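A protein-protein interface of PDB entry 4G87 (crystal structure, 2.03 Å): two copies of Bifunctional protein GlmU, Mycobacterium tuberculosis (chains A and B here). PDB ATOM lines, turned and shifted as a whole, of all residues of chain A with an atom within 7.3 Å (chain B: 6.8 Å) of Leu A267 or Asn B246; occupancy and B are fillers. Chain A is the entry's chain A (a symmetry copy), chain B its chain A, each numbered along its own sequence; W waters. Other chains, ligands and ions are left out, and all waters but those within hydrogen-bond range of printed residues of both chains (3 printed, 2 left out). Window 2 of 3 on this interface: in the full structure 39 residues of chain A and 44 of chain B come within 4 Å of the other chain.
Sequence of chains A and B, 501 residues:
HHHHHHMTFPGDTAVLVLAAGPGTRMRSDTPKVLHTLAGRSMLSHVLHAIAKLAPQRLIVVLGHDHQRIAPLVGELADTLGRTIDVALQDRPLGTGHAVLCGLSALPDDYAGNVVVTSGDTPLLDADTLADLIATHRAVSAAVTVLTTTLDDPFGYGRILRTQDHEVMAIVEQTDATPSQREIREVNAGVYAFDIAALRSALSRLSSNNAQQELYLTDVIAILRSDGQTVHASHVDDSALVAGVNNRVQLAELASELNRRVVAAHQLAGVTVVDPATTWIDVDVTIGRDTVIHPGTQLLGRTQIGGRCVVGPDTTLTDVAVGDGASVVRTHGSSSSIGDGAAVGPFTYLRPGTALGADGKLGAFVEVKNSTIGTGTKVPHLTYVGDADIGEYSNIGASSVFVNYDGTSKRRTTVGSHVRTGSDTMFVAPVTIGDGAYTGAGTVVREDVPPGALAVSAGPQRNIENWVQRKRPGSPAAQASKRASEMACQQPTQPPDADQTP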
ATOM      1  N   VAL A 261      18.731  22.186 -13.620  1.00  0.00           N
ATOM      2  CA  VAL A 261      19.954  22.118 -14.342  1.00  0.00           C
ATOM      3  C   VAL A 261      20.553  20.662 -14.214  1.00  0.00           C
ATOM      4  O   VAL A 261      20.991  20.035 -15.211  1.00  0.00           O
ATOM      5  CB  VAL A 261      20.981  23.140 -13.844  1.00  0.00           C
ATOM      6  CG1 VAL A 261      22.420  22.876 -14.464  1.00  0.00           C
ATOM      7  CG2 VAL A 261      20.528  24.666 -14.106  1.00  0.00           C
ATOM      8  N   VAL A 262      20.570  20.144 -13.021  1.00  0.00           N
ATOM      9  CA  VAL A 262      21.079  18.776 -12.808  1.00  0.00           C
ATOM     10  C   VAL A 262      20.232  17.805 -13.624  1.00  0.00           C
ATOM     11  O   VAL A 262      20.803  16.878 -14.213  1.00  0.00           O
ATOM     12  CB  VAL A 262      20.980  18.390 -11.280  1.00  0.00           C
ATOM     13  CG1 VAL A 262      21.207  16.896 -11.057  1.00  0.00           C
ATOM     14  CG2 VAL A 262      22.052  19.236 -10.444  1.00  0.00           C
ATOM     15  N   ALA A 263      18.876  17.933 -13.540  1.00  0.00           N
ATOM     16  CA  ALA A 263      17.985  17.046 -14.311  1.00  0.00           C
ATOM     17  C   ALA A 263      18.289  17.035 -15.824  1.00  0.00           C
ATOM     18  O   ALA A 263      18.319  15.932 -16.436  1.00  0.00           O
ATOM     19  CB  ALA A 263      16.441  17.300 -14.032  1.00  0.00           C
ATOM     20  N   ALA A 264      18.517  18.219 -16.421  1.00  0.00           N
ATOM     21  CA  ALA A 264      18.912  18.266 -17.809  1.00  0.00           C
ATOM     22  C   ALA A 264      20.202  17.498 -18.088  1.00  0.00           C
ATOM     23  O   ALA A 264      20.302  16.819 -19.137  1.00  0.00           O
ATOM     24  CB  ALA A 264      19.066  19.721 -18.302  1.00  0.00           C
ATOM     25  N   HIS A 265      21.209  17.621 -17.230  1.00  0.00           N
ATOM     26  CA  HIS A 265      22.406  16.786 -17.369  1.00  0.00           C
ATOM     27  C   HIS A 265      22.144  15.282 -17.200  1.00  0.00           C
ATOM     28  O   HIS A 265      22.673  14.471 -18.008  1.00  0.00           O
ATOM     29  CB  HIS A 265      23.515  17.209 -16.393  1.00  0.00           C
ATOM     30  CG  HIS A 265      24.110  18.544 -16.731  1.00  0.00           C
ATOM     31  ND1 HIS A 265      24.875  18.758 -17.860  1.00  0.00           N
ATOM     32  CD2 HIS A 265      24.023  19.741 -16.101  1.00  0.00           C
ATOM     33  CE1 HIS A 265      25.264  20.018 -17.899  1.00  0.00           C
ATOM     34  NE2 HIS A 265      24.768  20.635 -16.833  1.00  0.00           N
ATOM     35  N   GLN A 266      21.345  14.890 -16.204  1.00  0.00           N
ATOM     36  CA  GLN A 266      20.987  13.494 -16.027  1.00  0.00           C
ATOM     37  C   GLN A 266      20.314  12.917 -17.281  1.00  0.00           C
ATOM     38  O   GLN A 266      20.668  11.826 -17.718  1.00  0.00           O
ATOM     39  CB  GLN A 266      20.039  13.324 -14.823  1.00  0.00           C
ATOM     40  CG  GLN A 266      20.742  13.690 -13.466  1.00  0.00           C
ATOM     41  CD  GLN A 266      19.730  13.636 -12.338  1.00  0.00           C
ATOM     42  OE1 GLN A 266      18.727  14.355 -12.363  1.00  0.00           O
ATOM     43  NE2 GLN A 266      20.000  12.793 -11.344  1.00  0.00           N
ATOM     44  N   LEU A 267      19.344  13.641 -17.843  1.00  0.00           N
ATOM     45  CA  LEU A 267      18.632  13.155 -19.021  1.00  0.00           C
ATOM     46  C   LEU A 267      19.590  13.108 -20.243  1.00  0.00           C
ATOM     47  O   LEU A 267      19.371  12.308 -21.161  1.00  0.00           O
ATOM     48  CB  LEU A 267      17.419  14.069 -19.316  1.00  0.00           C
ATOM     49  CG  LEU A 267      16.231  13.944 -18.338  1.00  0.00           C
ATOM     50  CD1 LEU A 267      15.134  14.934 -18.778  1.00  0.00           C
ATOM     51  CD2 LEU A 267      15.672  12.514 -18.269  1.00  0.00           C
ATOM     52  N   ALA A 268      20.643  13.935 -20.250  1.00  0.00           N
ATOM     53  CA  ALA A 268      21.634  13.911 -21.340  1.00  0.00           C
ATOM     54  C   ALA A 268      22.725  12.832 -21.134  1.00  0.00           C
ATOM     55  O   ALA A 268      23.575  12.611 -22.000  1.00  0.00           O
ATOM     56  CB  ALA A 268      22.275  15.331 -21.543  1.00  0.00           C
ATOM     57  N   GLY A 269      22.708  12.132 -20.022  1.00  0.00           N
ATOM     58  CA  GLY A 269      23.670  11.056 -19.856  1.00  0.00           C
ATOM     59  C   GLY A 269      24.684  11.220 -18.736  1.00  0.00           C
ATOM     60  O   GLY A 269      25.703  10.477 -18.699  1.00  0.00           O
ATOM     61  N   VAL A 270      24.411  12.131 -17.795  1.00  0.00           N
ATOM     62  CA  VAL A 270      25.330  12.325 -16.684  1.00  0.00           C
ATOM     63  C   VAL A 270      24.715  11.690 -15.407  1.00  0.00           C
ATOM     64  O   VAL A 270      23.581  12.004 -15.037  1.00  0.00           O
ATOM     65  CB  VAL A 270      25.591  13.819 -16.454  1.00  0.00           C
ATOM     66  CG1 VAL A 270      26.515  14.076 -15.190  1.00  0.00           C
ATOM     67  CG2 VAL A 270      26.203  14.478 -17.750  1.00  0.00           C
ATOM     68  N   THR B  24      17.750   2.913 -23.890  1.00  0.00           N
ATOM     69  CA  THR B  24      18.190   4.117 -24.622  1.00  0.00           C
ATOM     70  C   THR B  24      18.045   5.412 -23.765  1.00  0.00           C
ATOM     71  O   THR B  24      18.864   6.321 -23.866  1.00  0.00           O
ATOM     72  CB  THR B  24      17.456   4.258 -25.942  1.00  0.00           C
ATOM     73  OG1 THR B  24      16.037   4.372 -25.675  1.00  0.00           O
ATOM     74  CG2 THR B  24      17.722   2.942 -26.758  1.00  0.00           C
ATOM     75  N   ARG B  25      17.033   5.449 -22.907  1.00  0.00           N
ATOM     76  CA  ARG B  25      16.722   6.668 -22.131  1.00  0.00           C
ATOM     77  C   ARG B  25      17.757   6.936 -21.033  1.00  0.00           C
ATOM     78  O   ARG B  25      17.916   8.073 -20.552  1.00  0.00           O
ATOM     79  CB  ARG B  25      15.275   6.616 -21.637  1.00  0.00           C
ATOM     80  CG  ARG B  25      14.226   6.942 -22.818  1.00  0.00           C
ATOM     81  CD  ARG B  25      12.795   6.777 -22.259  1.00  0.00           C
ATOM     82  NE  ARG B  25      12.572   5.323 -21.999  1.00  0.00           N
ATOM     83  CZ  ARG B  25      11.452   4.817 -21.466  1.00  0.00           C
ATOM     84  NH1 ARG B  25      10.440   5.628 -21.066  1.00  0.00           N
ATOM     85  NH2 ARG B  25      11.325   3.507 -21.337  1.00  0.00           N
ATOM     86  N   MET B  26      18.532   5.911 -20.700  1.00  0.00           N
ATOM     87  CA  MET B  26      19.684   6.153 -19.795  1.00  0.00           C
ATOM     88  C   MET B  26      20.798   6.943 -20.456  1.00  0.00           C
ATOM     89  O   MET B  26      21.608   7.545 -19.743  1.00  0.00           O
ATOM     90  CB  MET B  26      20.268   4.853 -19.264  1.00  0.00           C
ATOM     91  CG  MET B  26      19.242   3.992 -18.548  1.00  0.00           C
ATOM     92  SD  MET B  26      18.676   4.675 -16.964  1.00  0.00           S
ATOM     93  CE  MET B  26      20.209   4.424 -15.966  1.00  0.00           C
ATOM     94  N   ARG B  27      20.892   6.911 -21.797  1.00  0.00           N
ATOM     95  CA  ARG B  27      21.994   7.645 -22.519  1.00  0.00           C
ATOM     96  C   ARG B  27      23.339   7.259 -21.943  1.00  0.00           C
ATOM     97  O   ARG B  27      24.150   8.109 -21.510  1.00  0.00           O
ATOM     98  CB  ARG B  27      21.788   9.155 -22.397  1.00  0.00           C
ATOM     99  CG  ARG B  27      20.521   9.684 -23.059  1.00  0.00           C
ATOM    100  CD  ARG B  27      20.823  10.032 -24.461  1.00  0.00           C
ATOM    101  NE  ARG B  27      20.255  11.329 -24.799  1.00  0.00           N
ATOM    102  CZ  ARG B  27      18.975  11.519 -25.111  1.00  0.00           C
ATOM    103  NH1 ARG B  27      18.113  10.497 -25.108  1.00  0.00           N
ATOM    104  NH2 ARG B  27      18.551  12.744 -25.400  1.00  0.00           N
ATOM    105  N   LYS B  32      21.713  -0.484 -18.921  1.00  0.00           N
ATOM    106  CA  LYS B  32      20.797   0.077 -17.922  1.00  0.00           C
ATOM    107  C   LYS B  32      20.784  -0.699 -16.611  1.00  0.00           C
ATOM    108  O   LYS B  32      20.857  -0.134 -15.516  1.00  0.00           O
ATOM    109  CB  LYS B  32      19.335   0.172 -18.441  1.00  0.00           C
ATOM    110  CG  LYS B  32      18.285   0.376 -17.294  1.00  0.00           C
ATOM    111  CD  LYS B  32      16.959   1.191 -17.645  1.00  0.00           C
ATOM    112  CE  LYS B  32      15.800   0.326 -18.102  1.00  0.00           C
ATOM    113  NZ  LYS B  32      14.609   1.192 -18.271  1.00  0.00           N
ATOM    114  N   PHE B 154       3.824   9.916 -15.057  1.00  0.00           N
ATOM    115  CA  PHE B 154       4.430  10.042 -16.391  1.00  0.00           C
ATOM    116  C   PHE B 154       5.215   8.812 -16.794  1.00  0.00           C
ATOM    117  O   PHE B 154       6.087   8.324 -16.052  1.00  0.00           O
ATOM    118  CB  PHE B 154       5.322  11.301 -16.503  1.00  0.00           C
ATOM    119  CG  PHE B 154       5.934  11.469 -17.887  1.00  0.00           C
ATOM    120  CD1 PHE B 154       7.243  11.090 -18.139  1.00  0.00           C
ATOM    121  CD2 PHE B 154       5.161  11.941 -18.949  1.00  0.00           C
ATOM    122  CE1 PHE B 154       7.794  11.201 -19.445  1.00  0.00           C
ATOM    123  CE2 PHE B 154       5.714  12.059 -20.253  1.00  0.00           C
ATOM    124  CZ  PHE B 154       7.016  11.689 -20.483  1.00  0.00           C
ATOM    125  N   GLY B 243       9.652   2.368 -11.142  1.00  0.00           N
ATOM    126  CA  GLY B 243      10.566   1.918 -12.221  1.00  0.00           C
ATOM    127  C   GLY B 243      11.622   2.981 -12.488  1.00  0.00           C
ATOM    128  O   GLY B 243      11.482   4.163 -12.056  1.00  0.00           O
ATOM    129  N   VAL B 244      12.667   2.572 -13.202  1.00  0.00           N
ATOM    130  CA  VAL B 244      13.795   3.467 -13.553  1.00  0.00           C
ATOM    131  C   VAL B 244      14.062   3.413 -15.034  1.00  0.00           C
ATOM    132  O   VAL B 244      14.589   2.423 -15.491  1.00  0.00           O
ATOM    133  CB  VAL B 244      15.108   3.073 -12.807  1.00  0.00           C
ATOM    134  CG1 VAL B 244      16.268   3.946 -13.216  1.00  0.00           C
ATOM    135  CG2 VAL B 244      14.879   3.198 -11.282  1.00  0.00           C
ATOM    136  N   ASN B 245      13.652   4.450 -15.769  1.00  0.00           N
ATOM    137  CA  ASN B 245      13.922   4.539 -17.215  1.00  0.00           C
ATOM    138  C   ASN B 245      15.039   5.488 -17.564  1.00  0.00           C
ATOM    139  O   ASN B 245      15.502   5.501 -18.677  1.00  0.00           O
ATOM    140  CB  ASN B 245      12.587   4.893 -17.980  1.00  0.00           C
ATOM    141  CG  ASN B 245      11.662   3.682 -18.018  1.00  0.00           C
ATOM    142  OD1 ASN B 245      12.178   2.594 -17.777  1.00  0.00           O
ATOM    143  ND2 ASN B 245      10.297   3.865 -18.108  1.00  0.00           N
ATOM    144  N   ASN B 246      15.441   6.344 -16.615  1.00  0.00           N
ATOM    145  CA  ASN B 246      16.429   7.371 -16.946  1.00  0.00           C
ATOM    146  C   ASN B 246      17.146   7.710 -15.620  1.00  0.00           C
ATOM    147  O   ASN B 246      16.751   7.239 -14.568  1.00  0.00           O
ATOM    148  CB  ASN B 246      15.781   8.641 -17.588  1.00  0.00           C
ATOM    149  CG  ASN B 246      14.747   9.320 -16.665  1.00  0.00           C
ATOM    150  OD1 ASN B 246      15.015   9.557 -15.469  1.00  0.00           O
ATOM    151  ND2 ASN B 246      13.614   9.679 -17.216  1.00  0.00           N
ATOM    152  N   ARG B 247      18.173   8.530 -15.717  1.00  0.00           N
ATOM    153  CA  ARG B 247      19.023   8.866 -14.614  1.00  0.00           C
ATOM    154  C   ARG B 247      18.372   9.735 -13.564  1.00  0.00           C
ATOM    155  O   ARG B 247      18.877   9.794 -12.406  1.00  0.00           O
ATOM    156  CB  ARG B 247      20.256   9.532 -15.181  1.00  0.00           C
ATOM    157  CG  ARG B 247      21.223   8.400 -15.800  1.00  0.00           C
ATOM    158  CD  ARG B 247      22.643   8.858 -15.912  1.00  0.00           C
ATOM    159  NE  ARG B 247      23.112   8.491 -17.180  1.00  0.00           N
ATOM    160  CZ  ARG B 247      24.282   7.990 -17.522  1.00  0.00           C
ATOM    161  NH1 ARG B 247      25.260   7.732 -16.677  1.00  0.00           N
ATOM    162  NH2 ARG B 247      24.429   7.751 -18.823  1.00  0.00           N
ATOM    163  N   VAL B 248      17.366  10.512 -13.971  1.00  0.00           N
ATOM    164  CA  VAL B 248      16.599  11.284 -13.005  1.00  0.00           C
ATOM    165  C   VAL B 248      15.854  10.333 -12.050  1.00  0.00           C
ATOM    166  O   VAL B 248      15.890  10.511 -10.822  1.00  0.00           O
ATOM    167  CB  VAL B 248      15.553  12.208 -13.683  1.00  0.00           C
ATOM    168  CG1 VAL B 248      14.651  12.874 -12.640  1.00  0.00           C
ATOM    169  CG2 VAL B 248      16.254  13.241 -14.668  1.00  0.00           C
ATOM    170  N   GLN B 249      15.144   9.351 -12.624  1.00  0.00           N
ATOM    171  CA  GLN B 249      14.432   8.358 -11.810  1.00  0.00           C
ATOM    172  C   GLN B 249      15.384   7.493 -10.993  1.00  0.00           C
ATOM    173  O   GLN B 249      15.065   7.116  -9.867  1.00  0.00           O
ATOM    174  CB  GLN B 249      13.546   7.456 -12.711  1.00  0.00           C
ATOM    175  CG  GLN B 249      12.465   8.287 -13.429  1.00  0.00           C
ATOM    176  CD  GLN B 249      11.494   7.434 -14.168  1.00  0.00           C
ATOM    177  OE1 GLN B 249      11.875   6.435 -14.753  1.00  0.00           O
ATOM    178  NE2 GLN B 249      10.219   7.826 -14.145  1.00  0.00           N
ATOM    179  N   LEU B 250      16.534   7.152 -11.567  1.00  0.00           N
ATOM    180  CA  LEU B 250      17.539   6.343 -10.877  1.00  0.00           C
ATOM    181  C   LEU B 250      17.949   7.109  -9.554  1.00  0.00           C
ATOM    182  O   LEU B 250      17.929   6.527  -8.426  1.00  0.00           O
ATOM    183  CB  LEU B 250      18.761   6.126 -11.817  1.00  0.00           C
ATOM    184  CG  LEU B 250      19.972   5.417 -11.143  1.00  0.00           C
ATOM    185  CD1 LEU B 250      19.539   4.093 -10.495  1.00  0.00           C
ATOM    186  CD2 LEU B 250      21.122   5.181 -12.049  1.00  0.00           C
ATOM    187  N   ALA B 251      18.255   8.398  -9.684  1.00  0.00           N
ATOM    188  CA  ALA B 251      18.694   9.188  -8.515  1.00  0.00           C
ATOM    189  C   ALA B 251      17.560   9.382  -7.508  1.00  0.00           C
ATOM    190  O   ALA B 251      17.790   9.345  -6.311  1.00  0.00           O
ATOM    191  CB  ALA B 251      19.268  10.528  -8.935  1.00  0.00           C
HETATM  192  O   HOH W   1      21.705  10.396 -11.839  1.00  0.00           O
HETATM  193  O   HOH W   2      19.041   9.540 -18.358  1.00  0.00           O
HETATM  194  O   HOH W   3      22.310  13.229 -25.029  1.00  0.00           O
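Printed residues of chain B that touch a printed residue of chain A: Arg B27, Asn B246, Arg B247, Val B248 and Ala B251. Of the 10 printed residues of chain A, 6 touch a printed residue of chain B. Hydrophobic or aromatic side chains of chain A that line the printed part of chain B: Leu A267. Among the printed residues, no Asp or Glu carboxylate lies within 4 Å of a Lys or Arg side-chain nitrogen of the other chain.
The backbone carbonyl oxygen of Arg B247 sits at hydrogen-bond distance from the side-chain amide nitrogen of Gln A266 (3.4 Å). O of Gly A269 sits at hydrogen-bond distance from NH2 of Arg B247, 3.0 Å away.
Among the printed residues, pairs that only touch across the chains: Ala A263 with Val B248, Gln A266 with Val B248, Gln A266 with Ala B251, Leu A267 with Arg B27, Leu A267 with Asn B246, Leu A267 with Val B248, Ala A268 with Arg B27, Gly A269 with Arg B27 and Val A270 with Arg B247.
Of chain B, only Arg B27 (3.4 Å), Asn B246 (3.7 Å) and Val B248 (3.7 Å) come within 4 Å of Leu A267. Of chain A, only Leu A267 (3.7 Å) comes within 4 Å of Asn B246. Printed residues of chain A within 4 Å of Arg B247: Gln A266, Gly A269 and Val A270. Printed residues of chain A within 4 Å of Ala B251: Gln A266 (3.4 Å). The nearest printed residue of chain B that does not touch Ala A263 is Arg B247 (6.8 Å).
No position is printed for both chains. Of the 11 pairs that touch across the chains among the printed residues, none has its exchanged pair printed and touching as well.
Water W3 lies within hydrogen-bond range of the guanidinium group of Arg B27 (2.8 Å) and the backbone carbonyl oxygen of Ala A268 (3.3 Å). Water W2 lies within hydrogen-bond range of the backbone carbonyl oxygen of Arg B25 (2.9 Å), the backbone carbonyl oxygen of Gln A266 (2.9 Å) and the backbone NH of Arg B247 (3.0 Å). Water W1 lies within hydrogen-bond range of O of Arg B247 (2.9 Å) and NE2 of Gln A266 (3.0 Å).
N of Asn B246 sits close to SD of Met B26. NH2 of Arg B247 is in hydrogen-bond range of O of Met B26, 3.0 Å away. The backbone carbonyl oxygen of Arg B27 lies within hydrogen-bond range of the guanidinium group of Arg B247 (2.7 Å). OD1 of Asn B246 sits at hydrogen-bond distance from N of Val B248 (2.9 Å). The side-chain amide oxygen (OD1) of Asn B246 lies within hydrogen-bond range of the backbone NH (N) of Gln B249 (2.9 Å). The backbone carbonyl oxygen (O) of His A265 lies within hydrogen-bond range of the backbone NH (N) of Val A270, 2.9 Å away.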
